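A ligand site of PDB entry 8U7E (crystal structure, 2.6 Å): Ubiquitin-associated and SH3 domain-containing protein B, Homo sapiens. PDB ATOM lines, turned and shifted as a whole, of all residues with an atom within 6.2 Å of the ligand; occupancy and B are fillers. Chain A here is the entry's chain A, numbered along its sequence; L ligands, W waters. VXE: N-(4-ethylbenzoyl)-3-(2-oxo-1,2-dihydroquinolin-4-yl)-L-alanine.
The guanidinium group of Arg 28 is in salt-bridge range of an oxygen (O20) of the ligand (3.3 Å). O20 of the ligand lies within salt-bridge range of NH1 of Arg 32, 3.1 Å away.
The side-chain carboxylate (OE2) of Glu 139 is in salt-bridge range of the guanidinium group (NH2) of Arg 111 (3.1 Å). A ring nitrogen (NE2) of His 29 sits at hydrogen-bond distance from the guanidinium group of Arg 111, at 3.3 Å. NH2 of Arg 32 lies within salt-bridge range of OD2 of Asp 34 (2.7 Å). The backbone NH of Glu 139 lies close to a ring nitrogen (NE2) of His 214 (3.4 Å).
The backbone carbonyl oxygen (O) of Trp 143 sits close to an oxygen (O01) of the ligand, at 3.4 Å. His 29 touches the ligand (NE2 to O20, 3.7 Å). Asp 34 touches the ligand. Val 35 touches the ligand. CA of Lys 39 touches C15 of the ligand (3.8 Å). Glu 139 touches the ligand (OE1 to C06, 3.3 Å). CB of Ala 215 touches O21 of the ligand, 3.9 Å away. CG1 of Val 237 touches C25 of the ligand, 3.6 Å away. Arg 241 touches the ligand. Hydrophobic or aromatic side chains within 4 Å of the ligand: Val 35, Trp 143, Ala 215 and Val 237.
Water W1 lies within hydrogen-bond range of O21 of the ligand (2.5 Å), NE of Arg 28 (2.6 Å), N of Ala 215 (2.8 Å) and NE2 of His 29 (2.9 Å).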
ATOM      1  N   ARG A  28     -31.639  -8.909  37.826  1.00  0.00           N
ATOM      2  CA  ARG A  28     -30.554  -8.897  36.872  1.00  0.00           C
ATOM      3  C   ARG A  28     -29.352  -8.205  37.463  1.00  0.00           C
ATOM      4  O   ARG A  28     -29.444  -7.421  38.402  1.00  0.00           O
ATOM      5  CB  ARG A  28     -31.062  -8.232  35.566  1.00  0.00           C
ATOM      6  CG  ARG A  28     -30.004  -7.636  34.636  1.00  0.00           C
ATOM      7  CD  ARG A  28     -30.605  -7.258  33.298  1.00  0.00           C
ATOM      8  NE  ARG A  28     -29.574  -7.212  32.269  1.00  0.00           N
ATOM      9  CZ  ARG A  28     -29.102  -6.122  31.670  1.00  0.00           C
ATOM     10  NH1 ARG A  28     -29.602  -4.924  31.958  1.00  0.00           N
ATOM     11  NH2 ARG A  28     -28.129  -6.268  30.780  1.00  0.00           N
ATOM     12  N   HIS A  29     -28.201  -8.554  36.956  1.00  0.00           N
ATOM     13  CA  HIS A  29     -26.958  -8.075  37.519  1.00  0.00           C
ATOM     14  C   HIS A  29     -26.855  -6.570  37.264  1.00  0.00           C
ATOM     15  O   HIS A  29     -27.696  -5.960  36.610  1.00  0.00           O
ATOM     16  CB  HIS A  29     -25.771  -8.861  36.934  1.00  0.00           C
ATOM     17  CG  HIS A  29     -25.696  -8.780  35.441  1.00  0.00           C
ATOM     18  ND1 HIS A  29     -25.182  -7.684  34.776  1.00  0.00           N
ATOM     19  CD2 HIS A  29     -26.192  -9.597  34.479  1.00  0.00           C
ATOM     20  CE1 HIS A  29     -25.338  -7.850  33.478  1.00  0.00           C
ATOM     21  NE2 HIS A  29     -25.935  -9.008  33.269  1.00  0.00           N
ATOM     22  N   ARG A  32     -22.258  -3.494  33.330  1.00  0.00           N
ATOM     23  CA  ARG A  32     -21.180  -4.340  32.788  1.00  0.00           C
ATOM     24  C   ARG A  32     -19.990  -3.520  32.301  1.00  0.00           C
ATOM     25  O   ARG A  32     -20.126  -2.651  31.405  1.00  0.00           O
ATOM     26  CB  ARG A  32     -21.676  -5.203  31.631  1.00  0.00           C
ATOM     27  CG  ARG A  32     -22.435  -6.420  32.053  1.00  0.00           C
ATOM     28  CD  ARG A  32     -23.005  -7.081  30.856  1.00  0.00           C
ATOM     29  NE  ARG A  32     -21.958  -7.685  30.044  1.00  0.00           N
ATOM     30  CZ  ARG A  32     -22.106  -8.823  29.367  1.00  0.00           C
ATOM     31  NH1 ARG A  32     -23.276  -9.483  29.394  1.00  0.00           N
ATOM     32  NH2 ARG A  32     -21.097  -9.287  28.650  1.00  0.00           N
ATOM     33  N   ASP A  34     -17.773  -4.350  30.244  1.00  0.00           N
ATOM     34  CA  ASP A  34     -17.584  -4.534  28.834  1.00  0.00           C
ATOM     35  C   ASP A  34     -18.730  -3.989  28.001  1.00  0.00           C
ATOM     36  O   ASP A  34     -18.792  -4.292  26.810  1.00  0.00           O
ATOM     37  CB  ASP A  34     -17.409  -6.031  28.544  1.00  0.00           C
ATOM     38  CG  ASP A  34     -18.636  -6.828  28.884  1.00  0.00           C
ATOM     39  OD1 ASP A  34     -19.470  -6.271  29.619  1.00  0.00           O
ATOM     40  OD2 ASP A  34     -18.765  -7.979  28.413  1.00  0.00           O
ATOM     41  N   VAL A  35     -19.657  -3.239  28.586  1.00  0.00           N
ATOM     42  CA  VAL A  35     -20.682  -2.515  27.847  1.00  0.00           C
ATOM     43  C   VAL A  35     -20.368  -1.031  27.807  1.00  0.00           C
ATOM     44  O   VAL A  35     -20.550  -0.367  26.786  1.00  0.00           O
ATOM     45  CB  VAL A  35     -22.084  -2.758  28.444  1.00  0.00           C
ATOM     46  CG1 VAL A  35     -23.121  -1.725  27.883  1.00  0.00           C
ATOM     47  CG2 VAL A  35     -22.593  -4.148  28.189  1.00  0.00           C
ATOM     48  N   GLY A  38     -16.696  -1.234  26.060  1.00  0.00           N
ATOM     49  CA  GLY A  38     -16.641  -1.918  24.772  1.00  0.00           C
ATOM     50  C   GLY A  38     -16.072  -3.321  24.813  1.00  0.00           C
ATOM     51  O   GLY A  38     -15.641  -3.839  25.845  1.00  0.00           O
ATOM     52  N   LYS A  39     -16.100  -3.970  23.646  1.00  0.00           N
ATOM     53  CA  LYS A  39     -15.549  -5.324  23.543  1.00  0.00           C
ATOM     54  C   LYS A  39     -14.046  -5.332  23.880  1.00  0.00           C
ATOM     55  O   LYS A  39     -13.543  -6.300  24.464  1.00  0.00           O
ATOM     56  CB  LYS A  39     -15.816  -5.898  22.151  1.00  0.00           C
ATOM     57  N   TRP A  41     -12.348  -3.321  26.089  1.00  0.00           N
ATOM     58  CA  TRP A  41     -12.046  -2.599  27.322  1.00  0.00           C
ATOM     59  C   TRP A  41     -10.695  -2.988  27.900  1.00  0.00           C
ATOM     60  O   TRP A  41      -9.935  -2.128  28.360  1.00  0.00           O
ATOM     61  CB  TRP A  41     -13.149  -2.852  28.332  1.00  0.00           C
ATOM     62  CG  TRP A  41     -13.367  -4.339  28.735  1.00  0.00           C
ATOM     63  CD1 TRP A  41     -13.978  -5.325  28.005  1.00  0.00           C
ATOM     64  CD2 TRP A  41     -12.994  -4.940  29.965  1.00  0.00           C
ATOM     65  NE1 TRP A  41     -14.022  -6.493  28.725  1.00  0.00           N
ATOM     66  CE2 TRP A  41     -13.434  -6.266  29.937  1.00  0.00           C
ATOM     67  CE3 TRP A  41     -12.363  -4.455  31.116  1.00  0.00           C
ATOM     68  CZ2 TRP A  41     -13.235  -7.125  30.981  1.00  0.00           C
ATOM     69  CZ3 TRP A  41     -12.180  -5.279  32.142  1.00  0.00           C
ATOM     70  CH2 TRP A  41     -12.608  -6.613  32.084  1.00  0.00           C
ATOM     71  N   GLU A  74     -12.255 -11.298  29.543  1.00  0.00           N
ATOM     72  CA  GLU A  74     -12.884 -10.848  28.304  1.00  0.00           C
ATOM     73  C   GLU A  74     -14.133 -11.646  27.947  1.00  0.00           C
ATOM     74  O   GLU A  74     -14.877 -11.218  27.060  1.00  0.00           O
ATOM     75  CB  GLU A  74     -11.888 -10.935  27.153  1.00  0.00           C
ATOM     76  CG  GLU A  74     -12.415 -10.307  25.867  1.00  0.00           C
ATOM     77  CD  GLU A  74     -11.496 -10.497  24.662  1.00  0.00           C
ATOM     78  OE1 GLU A  74     -10.424 -11.170  24.779  1.00  0.00           O
ATOM     79  OE2 GLU A  74     -11.872  -9.946  23.588  1.00  0.00           O
ATOM     80  N   ARG A 111     -20.009 -10.857  37.099  1.00  0.00           N
ATOM     81  CA  ARG A 111     -20.942  -9.758  37.194  1.00  0.00           C
ATOM     82  C   ARG A 111     -22.087 -10.074  38.159  1.00  0.00           C
ATOM     83  O   ARG A 111     -22.459  -9.227  38.980  1.00  0.00           O
ATOM     84  CB  ARG A 111     -21.379  -9.365  35.759  1.00  0.00           C
ATOM     85  CG  ARG A 111     -22.381 -10.240  35.001  1.00  0.00           C
ATOM     86  CD  ARG A 111     -22.545  -9.717  33.527  1.00  0.00           C
ATOM     87  NE  ARG A 111     -23.195 -10.684  32.631  1.00  0.00           N
ATOM     88  CZ  ARG A 111     -22.532 -11.670  32.015  1.00  0.00           C
ATOM     89  NH1 ARG A 111     -21.209 -11.808  32.147  1.00  0.00           N
ATOM     90  NH2 ARG A 111     -23.208 -12.530  31.272  1.00  0.00           N
ATOM     91  N   GLU A 139     -26.837 -17.303  31.820  1.00  0.00           N
ATOM     92  CA  GLU A 139     -27.692 -16.977  30.676  1.00  0.00           C
ATOM     93  C   GLU A 139     -27.621 -18.062  29.602  1.00  0.00           C
ATOM     94  O   GLU A 139     -26.668 -18.883  29.514  1.00  0.00           O
ATOM     95  CB  GLU A 139     -27.367 -15.613  30.046  1.00  0.00           C
ATOM     96  CG  GLU A 139     -25.900 -15.335  29.951  1.00  0.00           C
ATOM     97  CD  GLU A 139     -25.543 -14.088  29.160  1.00  0.00           C
ATOM     98  OE1 GLU A 139     -26.433 -13.223  28.955  1.00  0.00           O
ATOM     99  OE2 GLU A 139     -24.356 -13.964  28.780  1.00  0.00           O
ATOM    100  N   LYS A 142     -26.407 -19.734  23.901  1.00  0.00           N
ATOM    101  CA  LYS A 142     -26.233 -19.232  22.542  1.00  0.00           C
ATOM    102  C   LYS A 142     -25.651 -17.829  22.563  1.00  0.00           C
ATOM    103  O   LYS A 142     -25.209 -17.366  21.512  1.00  0.00           O
ATOM    104  CB  LYS A 142     -27.537 -19.279  21.772  1.00  0.00           C
ATOM    105  N   TRP A 143     -25.578 -17.172  23.735  1.00  0.00           N
ATOM    106  CA  TRP A 143     -24.984 -15.838  23.812  1.00  0.00           C
ATOM    107  C   TRP A 143     -23.510 -15.851  24.172  1.00  0.00           C
ATOM    108  O   TRP A 143     -22.922 -14.777  24.360  1.00  0.00           O
ATOM    109  CB  TRP A 143     -25.739 -14.953  24.806  1.00  0.00           C
ATOM    110  CG  TRP A 143     -27.079 -14.596  24.287  1.00  0.00           C
ATOM    111  CD1 TRP A 143     -27.469 -14.534  22.975  1.00  0.00           C
ATOM    112  CD2 TRP A 143     -28.243 -14.284  25.059  1.00  0.00           C
ATOM    113  NE1 TRP A 143     -28.780 -14.208  22.871  1.00  0.00           N
ATOM    114  CE2 TRP A 143     -29.289 -14.022  24.129  1.00  0.00           C
ATOM    115  CE3 TRP A 143     -28.497 -14.182  26.422  1.00  0.00           C
ATOM    116  CZ2 TRP A 143     -30.582 -13.644  24.537  1.00  0.00           C
ATOM    117  CZ3 TRP A 143     -29.798 -13.809  26.831  1.00  0.00           C
ATOM    118  CH2 TRP A 143     -30.816 -13.543  25.877  1.00  0.00           C
ATOM    119  N   VAL A 144     -22.899 -17.024  24.281  1.00  0.00           N
ATOM    120  CA  VAL A 144     -21.473 -17.100  24.618  1.00  0.00           C
ATOM    121  C   VAL A 144     -20.681 -17.060  23.330  1.00  0.00           C
ATOM    122  O   VAL A 144     -21.065 -17.678  22.325  1.00  0.00           O
ATOM    123  CB  VAL A 144     -21.159 -18.338  25.452  1.00  0.00           C
ATOM    124  CG1 VAL A 144     -19.694 -18.328  25.838  1.00  0.00           C
ATOM    125  CG2 VAL A 144     -21.998 -18.393  26.706  1.00  0.00           C
ATOM    126  N   HIS A 214     -29.323 -12.962  35.074  1.00  0.00           N
ATOM    127  CA  HIS A 214     -29.280 -12.198  33.829  1.00  0.00           C
ATOM    128  C   HIS A 214     -30.688 -11.724  33.473  1.00  0.00           C
ATOM    129  O   HIS A 214     -31.696 -12.206  33.993  1.00  0.00           O
ATOM    130  CB  HIS A 214     -28.674 -13.090  32.703  1.00  0.00           C
ATOM    131  CG  HIS A 214     -27.415 -13.773  33.128  1.00  0.00           C
ATOM    132  ND1 HIS A 214     -26.171 -13.254  32.839  1.00  0.00           N
ATOM    133  CD2 HIS A 214     -27.201 -14.868  33.905  1.00  0.00           C
ATOM    134  CE1 HIS A 214     -25.242 -14.005  33.395  1.00  0.00           C
ATOM    135  NE2 HIS A 214     -25.843 -14.977  34.059  1.00  0.00           N
ATOM    136  N   ALA A 215     -30.781 -10.807  32.532  1.00  0.00           N
ATOM    137  CA  ALA A 215     -32.105 -10.485  32.029  1.00  0.00           C
ATOM    138  C   ALA A 215     -32.843 -11.751  31.577  1.00  0.00           C
ATOM    139  O   ALA A 215     -34.029 -11.936  31.888  1.00  0.00           O
ATOM    140  CB  ALA A 215     -31.984  -9.425  30.938  1.00  0.00           C
ATOM    141  N   SER A 216     -32.130 -12.699  30.970  1.00  0.00           N
ATOM    142  CA  SER A 216     -32.802 -13.919  30.513  1.00  0.00           C
ATOM    143  C   SER A 216     -33.506 -14.581  31.659  1.00  0.00           C
ATOM    144  O   SER A 216     -34.566 -15.195  31.493  1.00  0.00           O
ATOM    145  CB  SER A 216     -31.774 -14.866  29.883  1.00  0.00           C
ATOM    146  N   VAL A 237     -36.952 -12.950  23.457  1.00  0.00           N
ATOM    147  CA  VAL A 237     -35.836 -12.015  23.371  1.00  0.00           C
ATOM    148  C   VAL A 237     -36.305 -10.583  23.368  1.00  0.00           C
ATOM    149  O   VAL A 237     -35.527  -9.668  23.640  1.00  0.00           O
ATOM    150  CB  VAL A 237     -34.980 -12.271  22.124  1.00  0.00           C
ATOM    151  CG1 VAL A 237     -33.758 -11.357  22.118  1.00  0.00           C
ATOM    152  CG2 VAL A 237     -34.615 -13.720  22.108  1.00  0.00           C
ATOM    153  N   VAL A 240     -36.728  -9.861  27.120  1.00  0.00           N
ATOM    154  CA  VAL A 240     -35.444  -9.831  27.802  1.00  0.00           C
ATOM    155  C   VAL A 240     -34.727  -8.520  27.598  1.00  0.00           C
ATOM    156  O   VAL A 240     -33.987  -8.064  28.480  1.00  0.00           O
ATOM    157  CB  VAL A 240     -34.578 -11.037  27.304  1.00  0.00           C
ATOM    158  CG1 VAL A 240     -33.112 -10.831  27.585  1.00  0.00           C
ATOM    159  CG2 VAL A 240     -35.152 -12.300  27.909  1.00  0.00           C
ATOM    160  N   ARG A 241     -34.868  -7.917  26.413  1.00  0.00           N
ATOM    161  CA  ARG A 241     -34.123  -6.684  26.142  1.00  0.00           C
ATOM    162  C   ARG A 241     -34.674  -5.492  26.898  1.00  0.00           C
ATOM    163  O   ARG A 241     -34.010  -4.450  26.944  1.00  0.00           O
ATOM    164  CB  ARG A 241     -34.109  -6.334  24.654  1.00  0.00           C
ATOM    165  CG  ARG A 241     -33.541  -7.434  23.712  1.00  0.00           C
ATOM    166  CD  ARG A 241     -32.025  -7.325  23.373  1.00  0.00           C
ATOM    167  NE  ARG A 241     -31.599  -5.986  22.896  1.00  0.00           N
ATOM    168  CZ  ARG A 241     -31.805  -5.502  21.660  1.00  0.00           C
ATOM    169  NH1 ARG A 241     -32.454  -6.218  20.769  1.00  0.00           N
ATOM    170  NH2 ARG A 241     -31.377  -4.301  21.316  1.00  0.00           N
ATOM    171  N   TYR A 245     -30.474  -2.911  34.175  1.00  0.00           N
ATOM    172  CA  TYR A 245     -29.557  -3.204  35.255  1.00  0.00           C
ATOM    173  C   TYR A 245     -30.306  -3.132  36.577  1.00  0.00           C
ATOM    174  O   TYR A 245     -31.019  -2.165  36.861  1.00  0.00           O
ATOM    175  CB  TYR A 245     -28.386  -2.208  35.213  1.00  0.00           C
ATOM    176  CG  TYR A 245     -27.431  -2.313  33.987  1.00  0.00           C
ATOM    177  CD1 TYR A 245     -27.209  -3.516  33.329  1.00  0.00           C
ATOM    178  CD2 TYR A 245     -26.770  -1.192  33.501  1.00  0.00           C
ATOM    179  CE1 TYR A 245     -26.305  -3.603  32.205  1.00  0.00           C
ATOM    180  CE2 TYR A 245     -25.940  -1.252  32.407  1.00  0.00           C
ATOM    181  CZ  TYR A 245     -25.666  -2.452  31.765  1.00  0.00           C
ATOM    182  OH  TYR A 245     -24.768  -2.499  30.684  1.00  0.00           O
HETATM  183  C11 VXE L   1     -22.728  -7.062  26.371  1.00  0.00           C
HETATM  184  C15 VXE L   1     -18.817  -6.979  24.696  1.00  0.00           C
HETATM  185  C14 VXE L   1     -19.445  -8.351  24.897  1.00  0.00           C
HETATM  186  C16 VXE L   1     -21.767  -9.336  25.009  1.00  0.00           C
HETATM  187  C19 VXE L   1     -27.222  -9.248  28.893  1.00  0.00           C
HETATM  188  C17 VXE L   1     -23.101  -9.232  25.378  1.00  0.00           C
HETATM  189  C02 VXE L   1     -25.534 -11.674  23.474  1.00  0.00           C
HETATM  190  C04 VXE L   1     -25.802 -11.465  24.936  1.00  0.00           C
HETATM  191  C05 VXE L   1     -27.125 -11.061  25.401  1.00  0.00           C
HETATM  192  C06 VXE L   1     -27.428 -10.848  26.885  1.00  0.00           C
HETATM  193  C07 VXE L   1     -27.030  -9.436  27.370  1.00  0.00           C
HETATM  194  C09 VXE L   1     -25.051  -8.043  26.440  1.00  0.00           C
HETATM  195  C10 VXE L   1     -23.579  -8.099  26.060  1.00  0.00           C
HETATM  196  C12 VXE L   1     -21.384  -7.150  25.987  1.00  0.00           C
HETATM  197  C13 VXE L   1     -20.911  -8.272  25.313  1.00  0.00           C
HETATM  198  C22 VXE L   1     -28.234 -10.811  24.375  1.00  0.00           C
HETATM  199  C23 VXE L   1     -27.984 -10.980  23.008  1.00  0.00           C
HETATM  200  C24 VXE L   1     -29.002 -10.760  22.075  1.00  0.00           C
HETATM  201  C25 VXE L   1     -30.270 -10.362  22.487  1.00  0.00           C
HETATM  202  C26 VXE L   1     -30.512 -10.188  23.852  1.00  0.00           C
HETATM  203  C27 VXE L   1     -29.502 -10.413  24.787  1.00  0.00           C
HETATM  204  N03 VXE L   1     -26.614 -11.432  22.499  1.00  0.00           N
HETATM  205  N08 VXE L   1     -25.648  -9.262  26.965  1.00  0.00           N
HETATM  206  O01 VXE L   1     -24.459 -12.024  23.065  1.00  0.00           O
HETATM  207  O18 VXE L   1     -25.673  -7.052  26.271  1.00  0.00           O
HETATM  208  O20 VXE L   1     -26.270  -8.787  29.635  1.00  0.00           O
HETATM  209  O21 VXE L   1     -28.362  -9.580  29.388  1.00  0.00           O
HETATM  210  O   HOH W   1     -28.416  -9.474  31.866  1.00  0.00           O
